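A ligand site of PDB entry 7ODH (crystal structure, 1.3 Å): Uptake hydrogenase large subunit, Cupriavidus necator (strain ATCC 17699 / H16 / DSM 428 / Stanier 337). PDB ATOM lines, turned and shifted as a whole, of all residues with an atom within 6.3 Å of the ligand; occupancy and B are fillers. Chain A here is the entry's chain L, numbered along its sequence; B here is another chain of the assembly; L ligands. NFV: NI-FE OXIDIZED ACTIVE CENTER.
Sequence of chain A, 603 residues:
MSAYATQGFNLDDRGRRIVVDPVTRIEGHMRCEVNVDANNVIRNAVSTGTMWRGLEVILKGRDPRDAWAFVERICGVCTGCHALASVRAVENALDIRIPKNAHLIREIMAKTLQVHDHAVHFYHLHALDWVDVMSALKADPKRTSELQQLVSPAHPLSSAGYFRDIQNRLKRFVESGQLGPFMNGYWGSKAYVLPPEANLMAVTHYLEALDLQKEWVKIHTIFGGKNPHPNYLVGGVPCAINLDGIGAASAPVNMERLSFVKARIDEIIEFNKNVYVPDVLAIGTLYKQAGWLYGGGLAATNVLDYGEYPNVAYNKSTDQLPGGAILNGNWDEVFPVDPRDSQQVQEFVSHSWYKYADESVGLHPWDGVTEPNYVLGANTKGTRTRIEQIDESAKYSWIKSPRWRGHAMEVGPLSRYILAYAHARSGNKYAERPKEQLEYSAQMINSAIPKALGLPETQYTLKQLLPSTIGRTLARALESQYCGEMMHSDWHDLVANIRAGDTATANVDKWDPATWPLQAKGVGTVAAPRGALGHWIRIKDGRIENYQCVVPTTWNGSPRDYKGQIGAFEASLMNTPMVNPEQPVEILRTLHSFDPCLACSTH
A nickel atom (NI) of the ligand is bound by the side-chain sulfur (SG) of Cys 597, 2.2 Å away.
NI of the ligand is bound by SG of Cys 75.
The side-chain sulfur (SG) of Cys 78 is bound to an iron atom (FE) of the ligand, at 2.3 Å.
The side-chain sulfur (SG) of Cys 600 binds an iron atom (FE) of the ligand.
The backbone NH (N) of Arg 530 is in hydrogen-bond range of a nitrogen (N3) of the ligand.
The guanidinium group (NH2) of Arg 530 lies within hydrogen-bond range of a nitrogen (N3) of the ligand.
N2 of the ligand sits at hydrogen-bond distance from N of Thr 553, at 3.0 Å.
A nitrogen (N2) of the ligand sits at hydrogen-bond distance from the side-chain hydroxyl (OG1) of Thr 553, 2.9 Å away.
A ring nitrogen (NE2) of His 82 sits at hydrogen-bond distance from an oxygen (O1) of the ligand, at 3.3 Å.
An oxygen (O1) of the ligand is in hydrogen-bond range of the side-chain sulfur (SG) of Cys 81 (3.3 Å).
SG of Cys 597 sits close to OE1 of Glu 27, 3.5 Å away.
SG of Cys 75 sits close to N of Val 77 (3.4 Å).
SG of Cys 81 is in hydrogen-bond range of O of Cys 78 (3.3 Å).
The side-chain sulfur of Cys 600 sits close to a ring nitrogen (NE2) of His 82.
The side-chain carboxylate of Asp 117 is in salt-bridge range of the guanidinium group of Arg 530.
NH1 of Arg 530 is in salt-bridge range of OD1 of Asp 595.
A ring nitrogen (ND1) of His 82 lies within hydrogen-bond range of a ring nitrogen (NE2) of His 535, at 2.9 Å.
O of Val 551 sits close to OG1 of Thr 554 (3.2 Å).
N3 of the ligand lies close to N of Pro 529.
Merely in contact with the ligand: Ala 528, Leu 533, Val 551 and Pro 552.
Hydrophobic or aromatic side chains within 4 Å of the ligand: His 82, Ala 528, Pro 529, Leu 533, Val 551 and Pro 552.
Along chain A the residues within 4 Å of the ligand span positions 75 to 600.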
ATOM      1  N   GLU A  27      31.519  -8.782 -21.159  1.00  0.00           N
ATOM      2  CA  GLU A  27      30.728  -9.615 -20.237  1.00  0.00           C
ATOM      3  C   GLU A  27      29.793 -10.477 -21.081  1.00  0.00           C
ATOM      4  O   GLU A  27      29.126  -9.958 -21.993  1.00  0.00           O
ATOM      5  CB  GLU A  27      29.987  -8.767 -19.212  1.00  0.00           C
ATOM      6  CG  GLU A  27      29.338  -9.595 -18.123  1.00  0.00           C
ATOM      7  CD  GLU A  27      28.191 -10.480 -18.578  1.00  0.00           C
ATOM      8  OE1 GLU A  27      27.505 -10.097 -19.535  1.00  0.00           O
ATOM      9  OE2 GLU A  27      27.990 -11.572 -17.970  1.00  0.00           O
ATOM     10  N   ILE A  74      21.218  -9.911 -12.689  1.00  0.00           N
ATOM     11  CA  ILE A  74      21.340  -9.746 -14.168  1.00  0.00           C
ATOM     12  C   ILE A  74      22.830  -9.609 -14.480  1.00  0.00           C
ATOM     13  O   ILE A  74      23.274 -10.093 -15.539  1.00  0.00           O
ATOM     14  CB  ILE A  74      20.504  -8.571 -14.667  1.00  0.00           C
ATOM     15  CG1 ILE A  74      19.016  -8.921 -14.602  1.00  0.00           C
ATOM     16  CG2 ILE A  74      20.934  -8.173 -16.072  1.00  0.00           C
ATOM     17  CD1 ILE A  74      18.094  -7.766 -14.855  1.00  0.00           C
ATOM     18  N   CYS A  75      23.598  -8.933 -13.636  1.00  0.00           N
ATOM     19  CA  CYS A  75      24.992  -8.615 -13.993  1.00  0.00           C
ATOM     20  C   CYS A  75      25.856  -8.309 -12.773  1.00  0.00           C
ATOM     21  O   CYS A  75      25.494  -7.438 -11.984  1.00  0.00           O
ATOM     22  CB  CYS A  75      25.028  -7.435 -14.946  1.00  0.00           C
ATOM     23  SG  CYS A  75      26.682  -7.236 -15.641  1.00  0.00           S
ATOM     24  N   GLY A  76      27.009  -8.968 -12.724  1.00  0.00           N
ATOM     25  CA  GLY A  76      28.005  -8.766 -11.661  1.00  0.00           C
ATOM     26  C   GLY A  76      29.087  -7.763 -12.032  1.00  0.00           C
ATOM     27  O   GLY A  76      29.920  -7.467 -11.180  1.00  0.00           O
ATOM     28  N   VAL A  77      29.095  -7.315 -13.288  1.00  0.00           N
ATOM     29  CA  VAL A  77      30.039  -6.263 -13.757  1.00  0.00           C
ATOM     30  C   VAL A  77      29.413  -4.903 -13.436  1.00  0.00           C
ATOM     31  O   VAL A  77      29.986  -4.167 -12.634  1.00  0.00           O
ATOM     32  CB  VAL A  77      30.378  -6.433 -15.240  1.00  0.00           C
ATOM     33  CG1 VAL A  77      31.332  -5.330 -15.713  1.00  0.00           C
ATOM     34  CG2 VAL A  77      30.976  -7.798 -15.503  1.00  0.00           C
ATOM     35  N   CYS A  78      28.210  -4.631 -13.950  1.00  0.00           N
ATOM     36  CA  CYS A  78      27.454  -3.400 -13.577  1.00  0.00           C
ATOM     37  C   CYS A  78      26.691  -3.682 -12.262  1.00  0.00           C
ATOM     38  O   CYS A  78      25.467  -3.459 -12.165  1.00  0.00           O
ATOM     39  CB  CYS A  78      26.608  -2.891 -14.734  1.00  0.00           C
ATOM     40  SG  CYS A  78      25.380  -4.059 -15.375  1.00  0.00           S
ATOM     41  N   THR A  79      27.408  -4.155 -11.254  1.00  0.00           N
ATOM     42  CA  THR A  79      26.797  -4.721 -10.030  1.00  0.00           C
ATOM     43  C   THR A  79      26.138  -3.601  -9.214  1.00  0.00           C
ATOM     44  O   THR A  79      26.805  -2.637  -8.808  1.00  0.00           O
ATOM     45  CB  THR A  79      27.805  -5.539  -9.221  1.00  0.00           C
ATOM     46  OG1 THR A  79      27.092  -6.047  -8.093  1.00  0.00           O
ATOM     47  CG2 THR A  79      28.998  -4.745  -8.748  1.00  0.00           C
ATOM     48  N   CYS A  81      23.520  -1.639 -10.242  1.00  0.00           N
ATOM     49  CA  CYS A  81      22.713  -0.651 -10.999  1.00  0.00           C
ATOM     50  C   CYS A  81      21.302  -1.213 -11.201  1.00  0.00           C
ATOM     51  O   CYS A  81      20.339  -0.417 -11.155  1.00  0.00           O
ATOM     52  CB  CYS A  81      23.365  -0.209 -12.299  1.00  0.00           C
ATOM     53  SG  CYS A  81      23.370  -1.423 -13.638  1.00  0.00           S
ATOM     54  N   HIS A  82      21.144  -2.520 -11.366  1.00  0.00           N
ATOM     55  CA  HIS A  82      19.803  -3.143 -11.488  1.00  0.00           C
ATOM     56  C   HIS A  82      19.076  -3.098 -10.150  1.00  0.00           C
ATOM     57  O   HIS A  82      17.853  -2.952 -10.126  1.00  0.00           O
ATOM     58  CB  HIS A  82      19.909  -4.581 -12.010  1.00  0.00           C
ATOM     59  CG  HIS A  82      20.273  -4.652 -13.449  1.00  0.00           C
ATOM     60  ND1 HIS A  82      19.402  -4.271 -14.453  1.00  0.00           N
ATOM     61  CD2 HIS A  82      21.429  -5.007 -14.044  1.00  0.00           C
ATOM     62  CE1 HIS A  82      20.016  -4.427 -15.612  1.00  0.00           C
ATOM     63  NE2 HIS A  82      21.252  -4.873 -15.391  1.00  0.00           N
ATOM     64  N   LEU A 113      30.386   2.598  -8.706  1.00  0.00           N
ATOM     65  CA  LEU A 113      30.262   1.601  -9.793  1.00  0.00           C
ATOM     66  C   LEU A 113      30.744   2.212 -11.105  1.00  0.00           C
ATOM     67  O   LEU A 113      31.482   1.553 -11.834  1.00  0.00           O
ATOM     68  CB  LEU A 113      28.813   1.123  -9.929  1.00  0.00           C
ATOM     69  CG  LEU A 113      28.610   0.150 -11.094  1.00  0.00           C
ATOM     70  CD1 LEU A 113      29.408  -1.126 -10.866  1.00  0.00           C
ATOM     71  CD2 LEU A 113      27.140  -0.152 -11.315  1.00  0.00           C
ATOM     72  N   ASP A 117      33.726   0.280 -12.919  1.00  0.00           N
ATOM     73  CA  ASP A 117      33.308  -0.370 -14.183  1.00  0.00           C
ATOM     74  C   ASP A 117      34.079   0.272 -15.354  1.00  0.00           C
ATOM     75  O   ASP A 117      34.691  -0.461 -16.151  1.00  0.00           O
ATOM     76  CB  ASP A 117      31.788  -0.300 -14.276  1.00  0.00           C
ATOM     77  CG  ASP A 117      31.171  -1.313 -15.187  1.00  0.00           C
ATOM     78  OD1 ASP A 117      31.869  -1.760 -16.113  1.00  0.00           O
ATOM     79  OD2 ASP A 117      29.980  -1.625 -14.984  1.00  0.00           O
ATOM     80  N   ALA A 528      23.165   3.888 -16.025  1.00  0.00           N
ATOM     81  CA  ALA A 528      24.086   2.778 -15.742  1.00  0.00           C
ATOM     82  C   ALA A 528      25.368   3.029 -16.525  1.00  0.00           C
ATOM     83  O   ALA A 528      25.378   3.826 -17.457  1.00  0.00           O
ATOM     84  CB  ALA A 528      23.420   1.475 -16.100  1.00  0.00           C
ATOM     85  N   PRO A 529      26.483   2.380 -16.140  1.00  0.00           N
ATOM     86  CA  PRO A 529      27.752   2.588 -16.837  1.00  0.00           C
ATOM     87  C   PRO A 529      27.669   2.537 -18.377  1.00  0.00           C
ATOM     88  O   PRO A 529      28.382   3.277 -19.024  1.00  0.00           O
ATOM     89  CB  PRO A 529      28.613   1.460 -16.270  1.00  0.00           C
ATOM     90  CG  PRO A 529      28.124   1.342 -14.838  1.00  0.00           C
ATOM     91  CD  PRO A 529      26.621   1.521 -14.962  1.00  0.00           C
ATOM     92  N   ARG A 530      26.804   1.696 -18.945  1.00  0.00           N
ATOM     93  CA  ARG A 530      26.758   1.482 -20.405  1.00  0.00           C
ATOM     94  C   ARG A 530      25.617   2.264 -21.062  1.00  0.00           C
ATOM     95  O   ARG A 530      25.514   2.194 -22.291  1.00  0.00           O
ATOM     96  CB  ARG A 530      26.659  -0.009 -20.707  1.00  0.00           C
ATOM     97  CG  ARG A 530      27.948  -0.751 -20.384  1.00  0.00           C
ATOM     98  CD  ARG A 530      27.734  -2.219 -20.114  1.00  0.00           C
ATOM     99  NE  ARG A 530      28.998  -2.774 -19.669  1.00  0.00           N
ATOM    100  CZ  ARG A 530      29.488  -2.683 -18.435  1.00  0.00           C
ATOM    101  NH1 ARG A 530      30.691  -3.142 -18.185  1.00  0.00           N
ATOM    102  NH2 ARG A 530      28.765  -2.171 -17.460  1.00  0.00           N
ATOM    103  N   GLY A 531      24.830   3.018 -20.309  1.00  0.00           N
ATOM    104  CA  GLY A 531      23.783   3.887 -20.876  1.00  0.00           C
ATOM    105  C   GLY A 531      22.481   3.837 -20.112  1.00  0.00           C
ATOM    106  O   GLY A 531      22.499   3.771 -18.876  1.00  0.00           O
ATOM    107  N   ALA A 532      21.363   3.898 -20.831  1.00  0.00           N
ATOM    108  CA  ALA A 532      20.024   4.117 -20.269  1.00  0.00           C
ATOM    109  C   ALA A 532      19.437   2.795 -19.788  1.00  0.00           C
ATOM    110  O   ALA A 532      19.151   1.913 -20.622  1.00  0.00           O
ATOM    111  CB  ALA A 532      19.158   4.775 -21.306  1.00  0.00           C
ATOM    112  N   LEU A 533      19.233   2.682 -18.478  1.00  0.00           N
ATOM    113  CA  LEU A 533      18.614   1.488 -17.849  1.00  0.00           C
ATOM    114  C   LEU A 533      17.220   1.855 -17.339  1.00  0.00           C
ATOM    115  O   LEU A 533      17.091   2.879 -16.643  1.00  0.00           O
ATOM    116  CB  LEU A 533      19.484   1.001 -16.691  1.00  0.00           C
ATOM    117  CG  LEU A 533      18.876  -0.110 -15.835  1.00  0.00           C
ATOM    118  CD1 LEU A 533      18.592  -1.362 -16.655  1.00  0.00           C
ATOM    119  CD2 LEU A 533      19.783  -0.450 -14.669  1.00  0.00           C
ATOM    120  N   HIS A 535      13.707  -0.237 -15.454  1.00  0.00           N
ATOM    121  CA  HIS A 535      12.870  -1.352 -14.962  1.00  0.00           C
ATOM    122  C   HIS A 535      11.435  -0.855 -14.846  1.00  0.00           C
ATOM    123  O   HIS A 535      11.221   0.178 -14.203  1.00  0.00           O
ATOM    124  CB  HIS A 535      13.333  -1.878 -13.603  1.00  0.00           C
ATOM    125  CG  HIS A 535      14.643  -2.574 -13.597  1.00  0.00           C
ATOM    126  ND1 HIS A 535      15.010  -3.385 -12.546  1.00  0.00           N
ATOM    127  CD2 HIS A 535      15.694  -2.567 -14.462  1.00  0.00           C
ATOM    128  CE1 HIS A 535      16.227  -3.854 -12.765  1.00  0.00           C
ATOM    129  NE2 HIS A 535      16.670  -3.355 -13.927  1.00  0.00           N
ATOM    130  N   VAL A 551      17.707  -2.573 -21.045  1.00  0.00           N
ATOM    131  CA  VAL A 551      19.038  -2.419 -20.432  1.00  0.00           C
ATOM    132  C   VAL A 551      19.939  -1.775 -21.476  1.00  0.00           C
ATOM    133  O   VAL A 551      19.661  -1.842 -22.683  1.00  0.00           O
ATOM    134  CB  VAL A 551      19.488  -3.792 -19.912  1.00  0.00           C
ATOM    135  CG1 VAL A 551      20.787  -3.747 -19.162  1.00  0.00           C
ATOM    136  CG2 VAL A 551      18.408  -4.434 -19.043  1.00  0.00           C
ATOM    137  N   PRO A 552      21.000  -1.034 -21.075  1.00  0.00           N
ATOM    138  CA  PRO A 552      21.733  -0.268 -22.087  1.00  0.00           C
ATOM    139  C   PRO A 552      22.235  -1.115 -23.267  1.00  0.00           C
ATOM    140  O   PRO A 552      22.128  -0.679 -24.410  1.00  0.00           O
ATOM    141  CB  PRO A 552      22.905   0.314 -21.284  1.00  0.00           C
ATOM    142  CG  PRO A 552      22.342   0.468 -19.881  1.00  0.00           C
ATOM    143  CD  PRO A 552      21.412  -0.721 -19.702  1.00  0.00           C
ATOM    144  N   THR A 553      22.802  -2.285 -22.993  1.00  0.00           N
ATOM    145  CA  THR A 553      23.352  -3.127 -24.066  1.00  0.00           C
ATOM    146  C   THR A 553      22.193  -3.726 -24.877  1.00  0.00           C
ATOM    147  O   THR A 553      22.411  -4.091 -26.030  1.00  0.00           O
ATOM    148  CB  THR A 553      24.363  -4.161 -23.544  1.00  0.00           C
ATOM    149  OG1 THR A 553      25.391  -3.467 -22.856  1.00  0.00           O
ATOM    150  CG2 THR A 553      24.981  -4.960 -24.669  1.00  0.00           C
ATOM    151  N   THR A 554      20.979  -3.779 -24.333  1.00  0.00           N
ATOM    152  CA  THR A 554      19.784  -4.121 -25.144  1.00  0.00           C
ATOM    153  C   THR A 554      19.657  -3.079 -26.268  1.00  0.00           C
ATOM    154  O   THR A 554      19.472  -3.453 -27.437  1.00  0.00           O
ATOM    155  CB  THR A 554      18.480  -4.170 -24.348  1.00  0.00           C
ATOM    156  OG1 THR A 554      18.680  -4.836 -23.094  1.00  0.00           O
ATOM    157  CG2 THR A 554      17.389  -4.856 -25.146  1.00  0.00           C
ATOM    158  N   ASP A 595      31.490  -1.172 -24.573  1.00  0.00           N
ATOM    159  CA  ASP A 595      31.558  -1.933 -23.307  1.00  0.00           C
ATOM    160  C   ASP A 595      30.369  -2.901 -23.254  1.00  0.00           C
ATOM    161  O   ASP A 595      29.509  -2.822 -22.376  1.00  0.00           O
ATOM    162  CB  ASP A 595      31.602  -0.909 -22.185  1.00  0.00           C
ATOM    163  CG  ASP A 595      31.660  -1.469 -20.793  1.00  0.00           C
ATOM    164  OD1 ASP A 595      31.984  -2.675 -20.623  1.00  0.00           O
ATOM    165  OD2 ASP A 595      31.367  -0.668 -19.880  1.00  0.00           O
ATOM    166  N   PRO A 596      30.242  -3.831 -24.223  1.00  0.00           N
ATOM    167  CA  PRO A 596      29.088  -4.723 -24.268  1.00  0.00           C
ATOM    168  C   PRO A 596      28.958  -5.575 -23.003  1.00  0.00           C
ATOM    169  O   PRO A 596      29.931  -6.201 -22.574  1.00  0.00           O
ATOM    170  CB  PRO A 596      29.348  -5.623 -25.474  1.00  0.00           C
ATOM    171  CG  PRO A 596      30.304  -4.817 -26.318  1.00  0.00           C
ATOM    172  CD  PRO A 596      31.185  -4.110 -25.320  1.00  0.00           C
ATOM    173  N   CYS A 597      27.769  -5.587 -22.442  1.00  0.00           N
ATOM    174  CA  CYS A 597      27.419  -6.488 -21.322  1.00  0.00           C
ATOM    175  C   CYS A 597      26.260  -7.369 -21.766  1.00  0.00           C
ATOM    176  O   CYS A 597      25.116  -6.898 -21.829  1.00  0.00           O
ATOM    177  CB  CYS A 597      27.072  -5.720 -20.069  1.00  0.00           C
ATOM    178  SG  CYS A 597      26.921  -6.804 -18.635  1.00  0.00           S
ATOM    179  N   LEU A 598      26.566  -8.600 -22.150  1.00  0.00           N
ATOM    180  CA  LEU A 598      25.577  -9.425 -22.862  1.00  0.00           C
ATOM    181  C   LEU A 598      24.578 -10.045 -21.873  1.00  0.00           C
ATOM    182  O   LEU A 598      23.411 -10.205 -22.246  1.00  0.00           O
ATOM    183  CB  LEU A 598      26.299 -10.451 -23.732  1.00  0.00           C
ATOM    184  CG  LEU A 598      26.681  -9.928 -25.111  1.00  0.00           C
ATOM    185  CD1 LEU A 598      25.463  -9.750 -26.005  1.00  0.00           C
ATOM    186  CD2 LEU A 598      27.450  -8.608 -25.033  1.00  0.00           C
ATOM    187  N   ALA A 599      24.989 -10.320 -20.647  1.00  0.00           N
ATOM    188  CA  ALA A 599      24.065 -10.776 -19.587  1.00  0.00           C
ATOM    189  C   ALA A 599      23.054  -9.662 -19.316  1.00  0.00           C
ATOM    190  O   ALA A 599      21.858  -9.925 -19.230  1.00  0.00           O
ATOM    191  CB  ALA A 599      24.807 -11.164 -18.344  1.00  0.00           C
ATOM    192  N   CYS A 600      23.527  -8.413 -19.230  1.00  0.00           N
ATOM    193  CA  CYS A 600      22.627  -7.246 -19.134  1.00  0.00           C
ATOM    194  C   CYS A 600      21.664  -7.199 -20.330  1.00  0.00           C
ATOM    195  O   CYS A 600      20.468  -6.962 -20.126  1.00  0.00           O
ATOM    196  CB  CYS A 600      23.422  -5.949 -19.116  1.00  0.00           C
ATOM    197  SG  CYS A 600      23.700  -5.403 -17.430  1.00  0.00           S
ATOM    198  N   SER A 601      22.186  -7.365 -21.536  1.00  0.00           N
ATOM    199  CA  SER A 601      21.397  -7.103 -22.760  1.00  0.00           C
ATOM    200  C   SER A 601      20.194  -8.044 -22.828  1.00  0.00           C
ATOM    201  O   SER A 601      19.157  -7.649 -23.386  1.00  0.00           O
ATOM    202  CB  SER A 601      22.247  -7.197 -23.999  1.00  0.00           C
ATOM    203  OG  SER A 601      22.553  -8.557 -24.318  1.00  0.00           O
ATOM    204  N   CYS B  17      26.306 -14.171 -14.530  1.00  0.00           N
ATOM    205  CA  CYS B  17      26.294 -12.700 -14.427  1.00  0.00           C
ATOM    206  C   CYS B  17      27.740 -12.175 -14.334  1.00  0.00           C
ATOM    207  O   CYS B  17      27.899 -10.954 -14.407  1.00  0.00           O
ATOM    208  CB  CYS B  17      25.427 -12.255 -13.248  1.00  0.00           C
ATOM    209  SG  CYS B  17      26.339 -12.205 -11.695  1.00  0.00           S
HETATM  210 FE   NFV L   1      24.594  -3.252 -17.411  1.00  0.00          FE
HETATM  211 NI   NFV L   1      26.319  -5.502 -16.967  1.00  0.00          NI
HETATM  212  C1  NFV L   1      23.028  -2.409 -16.888  1.00  0.00           C
HETATM  213  O1  NFV L   1      22.063  -1.935 -16.653  1.00  0.00           O
HETATM  214  C2  NFV L   1      24.264  -2.996 -19.249  1.00  0.00           C
HETATM  215  N2  NFV L   1      24.059  -2.843 -20.367  1.00  0.00           N
HETATM  216  C3  NFV L   1      25.390  -1.553 -17.394  1.00  0.00           C
HETATM  217  N3  NFV L   1      25.896  -0.514 -17.351  1.00  0.00           N
HETATM  218  O4  NFV L   1      26.369  -3.982 -17.960  1.00  0.00           O
